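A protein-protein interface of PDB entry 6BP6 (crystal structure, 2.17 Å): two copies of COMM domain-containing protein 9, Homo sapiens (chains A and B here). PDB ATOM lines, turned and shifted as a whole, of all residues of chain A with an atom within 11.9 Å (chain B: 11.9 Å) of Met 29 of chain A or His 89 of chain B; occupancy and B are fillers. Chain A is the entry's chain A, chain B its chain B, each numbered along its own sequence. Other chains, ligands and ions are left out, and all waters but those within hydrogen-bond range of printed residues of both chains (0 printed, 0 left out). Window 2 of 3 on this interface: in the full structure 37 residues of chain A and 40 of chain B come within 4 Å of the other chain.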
ATOM      1  N   ASP A  18      19.872  20.102  29.454  1.00  0.00           N
ATOM      2  CA  ASP A  18      20.404  20.469  28.151  1.00  0.00           C
ATOM      3  C   ASP A  18      20.124  19.359  27.148  1.00  0.00           C
ATOM      4  O   ASP A  18      19.809  18.221  27.504  1.00  0.00           O
ATOM      5  CB  ASP A  18      21.921  20.716  28.222  1.00  0.00           C
ATOM      6  CG  ASP A  18      22.278  22.064  28.818  1.00  0.00           C
ATOM      7  OD1 ASP A  18      21.383  22.764  29.327  1.00  0.00           O
ATOM      8  OD2 ASP A  18      23.469  22.427  28.759  1.00  0.00           O
ATOM      9  N   ILE A  19      20.272  19.704  25.876  1.00  0.00           N
ATOM     10  CA  ILE A  19      20.283  18.746  24.779  1.00  0.00           C
ATOM     11  C   ILE A  19      21.661  18.807  24.139  1.00  0.00           C
ATOM     12  O   ILE A  19      22.119  19.887  23.746  1.00  0.00           O
ATOM     13  CB  ILE A  19      19.183  19.057  23.753  1.00  0.00           C
ATOM     14  CG1 ILE A  19      17.807  18.742  24.338  1.00  0.00           C
ATOM     15  CG2 ILE A  19      19.432  18.297  22.464  1.00  0.00           C
ATOM     16  CD1 ILE A  19      16.671  19.284  23.517  1.00  0.00           C
ATOM     17  N   LYS A  20      22.330  17.659  24.050  1.00  0.00           N
ATOM     18  CA  LYS A  20      23.648  17.603  23.438  1.00  0.00           C
ATOM     19  C   LYS A  20      23.652  16.577  22.313  1.00  0.00           C
ATOM     20  O   LYS A  20      22.703  15.808  22.130  1.00  0.00           O
ATOM     21  CB  LYS A  20      24.734  17.265  24.462  1.00  0.00           C
ATOM     22  CG  LYS A  20      24.656  15.860  25.008  1.00  0.00           C
ATOM     23  CD  LYS A  20      25.655  15.685  26.129  1.00  0.00           C
ATOM     24  CE  LYS A  20      25.634  14.276  26.690  1.00  0.00           C
ATOM     25  NZ  LYS A  20      26.540  14.194  27.873  1.00  0.00           N
ATOM     26  N   THR A  21      24.732  16.602  21.537  1.00  0.00           N
ATOM     27  CA  THR A  21      24.942  15.594  20.508  1.00  0.00           C
ATOM     28  C   THR A  21      25.392  14.292  21.157  1.00  0.00           C
ATOM     29  O   THR A  21      26.179  14.298  22.109  1.00  0.00           O
ATOM     30  CB  THR A  21      25.989  16.069  19.494  1.00  0.00           C
ATOM     31  OG1 THR A  21      25.496  17.217  18.792  1.00  0.00           O
ATOM     32  CG2 THR A  21      26.317  14.974  18.489  1.00  0.00           C
ATOM     33  N   SER A  22      24.864  13.176  20.662  1.00  0.00           N
ATOM     34  CA  SER A  22      25.286  11.869  21.140  1.00  0.00           C
ATOM     35  C   SER A  22      26.571  11.449  20.438  1.00  0.00           C
ATOM     36  O   SER A  22      26.766  11.715  19.249  1.00  0.00           O
ATOM     37  CB  SER A  22      24.192  10.828  20.907  1.00  0.00           C
ATOM     38  OG  SER A  22      24.513   9.596  21.530  1.00  0.00           O
ATOM     39  N   SER A  23      27.455  10.794  21.188  1.00  0.00           N
ATOM     40  CA  SER A  23      28.734  10.349  20.655  1.00  0.00           C
ATOM     41  C   SER A  23      28.717   8.904  20.184  1.00  0.00           C
ATOM     42  O   SER A  23      29.449   8.561  19.252  1.00  0.00           O
ATOM     43  CB  SER A  23      29.830  10.517  21.712  1.00  0.00           C
ATOM     44  OG  SER A  23      29.759  11.802  22.300  1.00  0.00           O
ATOM     45  N   ASP A  24      27.895   8.056  20.803  1.00  0.00           N
ATOM     46  CA  ASP A  24      27.831   6.642  20.459  1.00  0.00           C
ATOM     47  C   ASP A  24      26.776   6.329  19.409  1.00  0.00           C
ATOM     48  O   ASP A  24      26.821   5.249  18.806  1.00  0.00           O
ATOM     49  CB  ASP A  24      27.542   5.810  21.713  1.00  0.00           C
ATOM     50  CG  ASP A  24      28.276   6.325  22.935  1.00  0.00           C
ATOM     51  OD1 ASP A  24      29.415   6.816  22.782  1.00  0.00           O
ATOM     52  OD2 ASP A  24      27.712   6.246  24.047  1.00  0.00           O
ATOM     53  N   SER A  25      25.838   7.242  19.176  1.00  0.00           N
ATOM     54  CA  SER A  25      24.692   6.951  18.327  1.00  0.00           C
ATOM     55  C   SER A  25      25.101   6.869  16.862  1.00  0.00           C
ATOM     56  O   SER A  25      25.793   7.752  16.345  1.00  0.00           O
ATOM     57  CB  SER A  25      23.618   8.022  18.513  1.00  0.00           C
ATOM     58  OG  SER A  25      22.551   7.841  17.600  1.00  0.00           O
ATOM     59  N   ILE A  26      24.670   5.796  16.195  1.00  0.00           N
ATOM     60  CA  ILE A  26      24.805   5.724  14.744  1.00  0.00           C
ATOM     61  C   ILE A  26      23.905   6.757  14.083  1.00  0.00           C
ATOM     62  O   ILE A  26      24.313   7.452  13.145  1.00  0.00           O
ATOM     63  CB  ILE A  26      24.485   4.301  14.249  1.00  0.00           C
ATOM     64  CG1 ILE A  26      25.387   3.273  14.934  1.00  0.00           C
ATOM     65  CG2 ILE A  26      24.622   4.221  12.738  1.00  0.00           C
ATOM     66  CD1 ILE A  26      26.840   3.388  14.558  1.00  0.00           C
ATOM     67  N   SER A  27      22.671   6.881  14.568  1.00  0.00           N
ATOM     68  CA  SER A  27      21.697   7.816  14.022  1.00  0.00           C
ATOM     69  C   SER A  27      21.956   9.260  14.432  1.00  0.00           C
ATOM     70  O   SER A  27      21.175  10.138  14.049  1.00  0.00           O
ATOM     71  CB  SER A  27      20.288   7.402  14.452  1.00  0.00           C
ATOM     72  OG  SER A  27      20.233   7.187  15.852  1.00  0.00           O
ATOM     73  N   ARG A  28      23.012   9.523  15.205  1.00  0.00           N
ATOM     74  CA  ARG A  28      23.390  10.871  15.629  1.00  0.00           C
ATOM     75  C   ARG A  28      22.265  11.594  16.359  1.00  0.00           C
ATOM     76  O   ARG A  28      22.261  12.828  16.425  1.00  0.00           O
ATOM     77  CB  ARG A  28      23.859  11.718  14.442  1.00  0.00           C
ATOM     78  CG  ARG A  28      25.115  11.212  13.758  1.00  0.00           C
ATOM     79  CD  ARG A  28      25.351  11.976  12.468  1.00  0.00           C
ATOM     80  NE  ARG A  28      26.694  11.774  11.935  1.00  0.00           N
ATOM     81  CZ  ARG A  28      27.153  12.363  10.835  1.00  0.00           C
ATOM     82  NH1 ARG A  28      26.376  13.191  10.149  1.00  0.00           N
ATOM     83  NH2 ARG A  28      28.391  12.128  10.422  1.00  0.00           N
ATOM     84  N   MET A  29      21.302  10.852  16.900  1.00  0.00           N
ATOM     85  CA  MET A  29      20.181  11.450  17.611  1.00  0.00           C
ATOM     86  C   MET A  29      20.668  12.260  18.801  1.00  0.00           C
ATOM     87  O   MET A  29      21.533  11.816  19.551  1.00  0.00           O
ATOM     88  CB  MET A  29      19.200  10.371  18.081  1.00  0.00           C
ATOM     89  CG  MET A  29      18.479   9.634  16.963  1.00  0.00           C
ATOM     90  SD  MET A  29      17.217  10.757  15.989  1.00  0.00           S
ATOM     91  CE  MET A  29      16.267  11.530  17.508  1.00  0.00           C
ATOM     92  N   ALA A  30      20.119  13.459  18.963  1.00  0.00           N
ATOM     93  CA  ALA A  30      20.424  14.257  20.136  1.00  0.00           C
ATOM     94  C   ALA A  30      19.937  13.548  21.398  1.00  0.00           C
ATOM     95  O   ALA A  30      19.066  12.672  21.360  1.00  0.00           O
ATOM     96  CB  ALA A  30      19.787  15.639  20.022  1.00  0.00           C
ATOM     97  N   VAL A  31      20.515  13.929  22.531  1.00  0.00           N
ATOM     98  CA  VAL A  31      20.213  13.241  23.781  1.00  0.00           C
ATOM     99  C   VAL A  31      20.076  14.273  24.898  1.00  0.00           C
ATOM    100  O   VAL A  31      20.801  15.286  24.916  1.00  0.00           O
ATOM    101  CB  VAL A  31      21.284  12.177  24.087  1.00  0.00           C
ATOM    102  CG1 VAL A  31      22.643  12.820  24.337  1.00  0.00           C
ATOM    103  CG2 VAL A  31      20.867  11.290  25.251  1.00  0.00           C
ATOM    104  N   PRO A  32      19.133  14.084  25.818  1.00  0.00           N
ATOM    105  CA  PRO A  32      19.041  14.979  26.972  1.00  0.00           C
ATOM    106  C   PRO A  32      20.097  14.644  28.011  1.00  0.00           C
ATOM    107  O   PRO A  32      20.499  13.490  28.183  1.00  0.00           O
ATOM    108  CB  PRO A  32      17.631  14.717  27.523  1.00  0.00           C
ATOM    109  CG  PRO A  32      16.924  13.913  26.479  1.00  0.00           C
ATOM    110  CD  PRO A  32      17.984  13.166  25.748  1.00  0.00           C
ATOM    111  N   THR A  33      20.543  15.677  28.717  1.00  0.00           N
ATOM    112  CA  THR A  33      21.493  15.490  29.800  1.00  0.00           C
ATOM    113  C   THR A  33      21.167  16.477  30.910  1.00  0.00           C
ATOM    114  O   THR A  33      20.656  17.574  30.660  1.00  0.00           O
ATOM    115  CB  THR A  33      22.943  15.656  29.323  1.00  0.00           C
ATOM    116  OG1 THR A  33      23.837  15.338  30.397  1.00  0.00           O
ATOM    117  CG2 THR A  33      23.206  17.080  28.855  1.00  0.00           C
ATOM    118  N   GLU A  63      20.012   7.161  33.233  1.00  0.00           N
ATOM    119  CA  GLU A  63      20.250   5.921  33.962  1.00  0.00           C
ATOM    120  C   GLU A  63      20.956   6.184  35.285  1.00  0.00           C
ATOM    121  O   GLU A  63      20.606   5.591  36.315  1.00  0.00           O
ATOM    122  CB  GLU A  63      21.063   4.961  33.093  1.00  0.00           C
ATOM    123  CG  GLU A  63      21.827   5.635  31.956  1.00  0.00           C
ATOM    124  CD  GLU A  63      20.955   5.921  30.738  1.00  0.00           C
ATOM    125  OE1 GLU A  63      20.084   5.085  30.416  1.00  0.00           O
ATOM    126  OE2 GLU A  63      21.134   6.988  30.114  1.00  0.00           O
ATOM    127  N   MET B   1      30.752  20.797  19.589  1.00  0.00           N
ATOM    128  CA  MET B   1      30.987  19.426  19.156  1.00  0.00           C
ATOM    129  C   MET B   1      29.965  18.467  19.745  1.00  0.00           C
ATOM    130  O   MET B   1      28.918  18.882  20.245  1.00  0.00           O
ATOM    131  CB  MET B   1      32.392  18.961  19.547  1.00  0.00           C
ATOM    132  CG  MET B   1      33.531  19.598  18.769  1.00  0.00           C
ATOM    133  SD  MET B   1      35.245  18.812  19.281  1.00  0.00           S
ATOM    134  CE  MET B   1      36.421  19.768  18.051  1.00  0.00           C
ATOM    135  N   ALA B   2      30.289  17.179  19.679  1.00  0.00           N
ATOM    136  CA  ALA B   2      29.483  16.136  20.295  1.00  0.00           C
ATOM    137  C   ALA B   2      29.833  16.046  21.777  1.00  0.00           C
ATOM    138  O   ALA B   2      30.475  16.935  22.344  1.00  0.00           O
ATOM    139  CB  ALA B   2      29.696  14.808  19.572  1.00  0.00           C
ATOM    140  N   ASN B   3      29.414  14.961  22.427  1.00  0.00           N
ATOM    141  CA  ASN B   3      29.739  14.735  23.834  1.00  0.00           C
ATOM    142  C   ASN B   3      31.041  13.942  23.914  1.00  0.00           C
ATOM    143  O   ASN B   3      31.060  12.713  24.026  1.00  0.00           O
ATOM    144  CB  ASN B   3      28.598  14.023  24.548  1.00  0.00           C
ATOM    145  CG  ASN B   3      28.966  13.597  25.961  1.00  0.00           C
ATOM    146  OD1 ASN B   3      28.960  14.407  26.890  1.00  0.00           O
ATOM    147  ND2 ASN B   3      29.285  12.319  26.126  1.00  0.00           N
ATOM    148  N   GLN B   4      32.153  14.668  23.827  1.00  0.00           N
ATOM    149  CA  GLN B   4      33.468  14.111  24.114  1.00  0.00           C
ATOM    150  C   GLN B   4      34.005  14.602  25.448  1.00  0.00           C
ATOM    151  O   GLN B   4      34.397  13.793  26.296  1.00  0.00           O
ATOM    152  CB  GLN B   4      34.457  14.450  22.989  1.00  0.00           C
ATOM    153  CG  GLN B   4      35.795  13.731  23.114  1.00  0.00           C
ATOM    154  CD  GLN B   4      35.652  12.220  23.066  1.00  0.00           C
ATOM    155  OE1 GLN B   4      34.897  11.681  22.256  1.00  0.00           O
ATOM    156  NE2 GLN B   4      36.375  11.527  23.941  1.00  0.00           N
ATOM    157  N   ALA B  81      10.422  14.217  29.548  1.00  0.00           N
ATOM    158  CA  ALA B  81       9.660  15.078  28.644  1.00  0.00           C
ATOM    159  C   ALA B  81      10.528  15.564  27.485  1.00  0.00           C
ATOM    160  O   ALA B  81      10.067  15.633  26.337  1.00  0.00           O
ATOM    161  CB  ALA B  81       9.063  16.262  29.408  1.00  0.00           C
ATOM    162  N   VAL B  82      11.792  15.899  27.762  1.00  0.00           N
ATOM    163  CA  VAL B  82      12.682  16.324  26.683  1.00  0.00           C
ATOM    164  C   VAL B  82      12.968  15.165  25.732  1.00  0.00           C
ATOM    165  O   VAL B  82      13.000  15.345  24.512  1.00  0.00           O
ATOM    166  CB  VAL B  82      13.976  16.931  27.255  1.00  0.00           C
ATOM    167  CG1 VAL B  82      15.035  17.050  26.170  1.00  0.00           C
ATOM    168  CG2 VAL B  82      13.692  18.298  27.857  1.00  0.00           C
ATOM    169  N   ALA B  83      13.179  13.960  26.271  1.00  0.00           N
ATOM    170  CA  ALA B  83      13.380  12.795  25.413  1.00  0.00           C
ATOM    171  C   ALA B  83      12.159  12.539  24.538  1.00  0.00           C
ATOM    172  O   ALA B  83      12.289  12.200  23.352  1.00  0.00           O
ATOM    173  CB  ALA B  83      13.699  11.569  26.269  1.00  0.00           C
ATOM    174  N   SER B  84      10.961  12.714  25.103  1.00  0.00           N
ATOM    175  CA  SER B  84       9.732  12.549  24.332  1.00  0.00           C
ATOM    176  C   SER B  84       9.648  13.573  23.207  1.00  0.00           C
ATOM    177  O   SER B  84       9.289  13.236  22.072  1.00  0.00           O
ATOM    178  CB  SER B  84       8.518  12.660  25.258  1.00  0.00           C
ATOM    179  OG  SER B  84       7.309  12.641  24.519  1.00  0.00           O
ATOM    180  N   LYS B  85       9.967  14.837  23.505  1.00  0.00           N
ATOM    181  CA  LYS B  85       9.948  15.853  22.454  1.00  0.00           C
ATOM    182  C   LYS B  85      11.012  15.583  21.400  1.00  0.00           C
ATOM    183  O   LYS B  85      10.828  15.931  20.230  1.00  0.00           O
ATOM    184  CB  LYS B  85      10.135  17.252  23.049  1.00  0.00           C
ATOM    185  CG  LYS B  85       8.922  17.789  23.796  1.00  0.00           C
ATOM    186  CD  LYS B  85       8.959  19.310  23.908  1.00  0.00           C
ATOM    187  CE  LYS B  85       8.551  19.990  22.603  1.00  0.00           C
ATOM    188  NZ  LYS B  85       7.090  19.863  22.319  1.00  0.00           N
ATOM    189  N   LEU B  86      12.130  14.966  21.790  1.00  0.00           N
ATOM    190  CA  LEU B  86      13.185  14.679  20.821  1.00  0.00           C
ATOM    191  C   LEU B  86      12.796  13.538  19.891  1.00  0.00           C
ATOM    192  O   LEU B  86      13.088  13.585  18.690  1.00  0.00           O
ATOM    193  CB  LEU B  86      14.490  14.357  21.542  1.00  0.00           C
ATOM    194  CG  LEU B  86      15.277  15.574  22.025  1.00  0.00           C
ATOM    195  CD1 LEU B  86      16.529  15.148  22.775  1.00  0.00           C
ATOM    196  CD2 LEU B  86      15.627  16.474  20.848  1.00  0.00           C
ATOM    197  N   GLU B  87      12.146  12.501  20.426  1.00  0.00           N
ATOM    198  CA  GLU B  87      11.701  11.402  19.575  1.00  0.00           C
ATOM    199  C   GLU B  87      10.644  11.844  18.571  1.00  0.00           C
ATOM    200  O   GLU B  87      10.498  11.207  17.523  1.00  0.00           O
ATOM    201  CB  GLU B  87      11.172  10.251  20.430  1.00  0.00           C
ATOM    202  CG  GLU B  87      12.076   9.025  20.433  1.00  0.00           C
ATOM    203  CD  GLU B  87      13.486   9.333  20.906  1.00  0.00           C
ATOM    204  OE1 GLU B  87      13.652  10.226  21.764  1.00  0.00           O
ATOM    205  OE2 GLU B  87      14.433   8.681  20.417  1.00  0.00           O
ATOM    206  N   HIS B  88       9.914  12.918  18.865  1.00  0.00           N
ATOM    207  CA  HIS B  88       8.975  13.519  17.920  1.00  0.00           C
ATOM    208  C   HIS B  88       9.707  14.639  17.191  1.00  0.00           C
ATOM    209  O   HIS B  88       9.761  15.781  17.651  1.00  0.00           O
ATOM    210  CB  HIS B  88       7.733  14.024  18.645  1.00  0.00           C
ATOM    211  CG  HIS B  88       6.893  14.957  17.827  1.00  0.00           C
ATOM    212  ND1 HIS B  88       6.272  14.572  16.658  1.00  0.00           N
ATOM    213  CD2 HIS B  88       6.578  16.261  18.008  1.00  0.00           C
ATOM    214  CE1 HIS B  88       5.609  15.597  16.156  1.00  0.00           C
ATOM    215  NE2 HIS B  88       5.777  16.635  16.956  1.00  0.00           N
ATOM    216  N   HIS B  89      10.286  14.306  16.042  1.00  0.00           N
ATOM    217  CA  HIS B  89      11.097  15.254  15.282  1.00  0.00           C
ATOM    218  C   HIS B  89      10.270  16.435  14.783  1.00  0.00           C
ATOM    219  O   HIS B  89      10.741  17.572  14.767  1.00  0.00           O
ATOM    220  CB  HIS B  89      11.770  14.554  14.100  1.00  0.00           C
ATOM    221  CG  HIS B  89      12.527  13.320  14.480  1.00  0.00           C
ATOM    222  ND1 HIS B  89      11.907  12.114  14.730  1.00  0.00           N
ATOM    223  CD2 HIS B  89      13.852  13.105  14.655  1.00  0.00           C
ATOM    224  CE1 HIS B  89      12.818  11.209  15.041  1.00  0.00           C
ATOM    225  NE2 HIS B  89      14.007  11.785  15.002  1.00  0.00           N
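Among the printed residues, merely in contact across the chains: Thr 21 of chain A with Ala 2 of chain B, Pro 32 of chain A with Val 82 of chain B, Ile 19 of chain A with Val 82 of chain B, Pro 32 of chain A with Ala 83 of chain B, Ala 30 of chain A with Leu 86 of chain B, Pro 32 of chain A with Leu 86 of chain B and Met 29 of chain A with Leu 86 of chain B.
No position is printed for both chains. Of the 11 pairs that touch across the chains among the printed residues, none has its exchanged pair printed and touching as well.
The backbone NH (N) of Val 31 of chain A lies within hydrogen-bond range of the backbone carbonyl oxygen (O) of Lys 20 of chain A. The backbone NH (N) of Met 29 of chain A is in hydrogen-bond range of the side-chain hydroxyl (OG) of Ser 25 of chain A (3.3 Å). O of Glu 87 of chain B is in hydrogen-bond range of ND1 of His 89 of chain B (3.3 Å).
Printed residues of chain B within 4 Å of Lys 20 of chain A: Asn 3. Thr 21 of chain A touches two residues of chain B. No residue of chain B comes within 4 Å of Ser 25 of chain A. No residue of chain B comes within 4 Å of Ser 27 of chain A. Arg 28 of chain A touches none of the printed residues of chain B. Of chain B, only Leu 86 (3.97 Å) and His 89 (3.4 Å) come within 4 Å of Met 29 of chain A. No residue of chain B comes within 4 Å of Val 31 of chain A. Of the printed residues of chain B, Pro 32 of chain A touches Val 82 (3.7 Å), Ala 83 (3.8 Å) and Leu 86 (3.9 Å). Of the printed residues of chain A, Ala 83 of chain B touches Pro 32 (3.8 Å). Ser 84 of chain B touches none of the printed residues of chain A. Of the printed residues of chain A, Leu 86 of chain B touches Met 29, Ala 30 and Pro 32. No residue of chain A comes within 4 Å of Glu 87 of chain B. No residue of chain A comes within 4 Å of His 88 of chain B. Of chain A, only Met 29 comes within 4 Å of His 89 of chain B. The nearest residue of chain B that does not touch Met 29 of chain A is Glu 87 of chain B (4.5 Å). The nearest residue of chain A that does not touch His 89 of chain B is Ser 27 of chain A (7.4 Å). The nearest printed residue of chain B that does not touch Pro 32 of chain A is Ser 84 of chain B (6.2 Å).
The side-chain amino group of Lys 20 of chain A lies within hydrogen-bond range of the side-chain amide oxygen of Asn 3 of chain B, at 2.6 Å. The backbone carbonyl oxygen (O) of Thr 21 of chain A sits at hydrogen-bond distance from the backbone NH (N) of Asn 3 of chain B (3.3 Å). The side-chain hydroxyl (OG) of Ser 23 of chain A lies close to the backbone NH (N) of Asn 3 of chain B, at 3.2 Å. NE2 of His 89 of chain B lies close to SD of Met 29 of chain A, 3.5 Å away.
Of the 17 printed residues of chain A, 7 touch a printed residue of chain B. Hydrophobic or aromatic side chains of chain A within 4 Å of the printed part of chain B: Ile 19, Met 29 and Pro 32. Hydrophobic or aromatic side chains of chain B within 4 Å of the printed part of chain A: Ala 2, Val 82, Ala 83, Leu 86 and His 89. Among the printed residues, no Asp or Glu carboxylate lies within 4 Å of a Lys or Arg side-chain nitrogen of the other chain.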
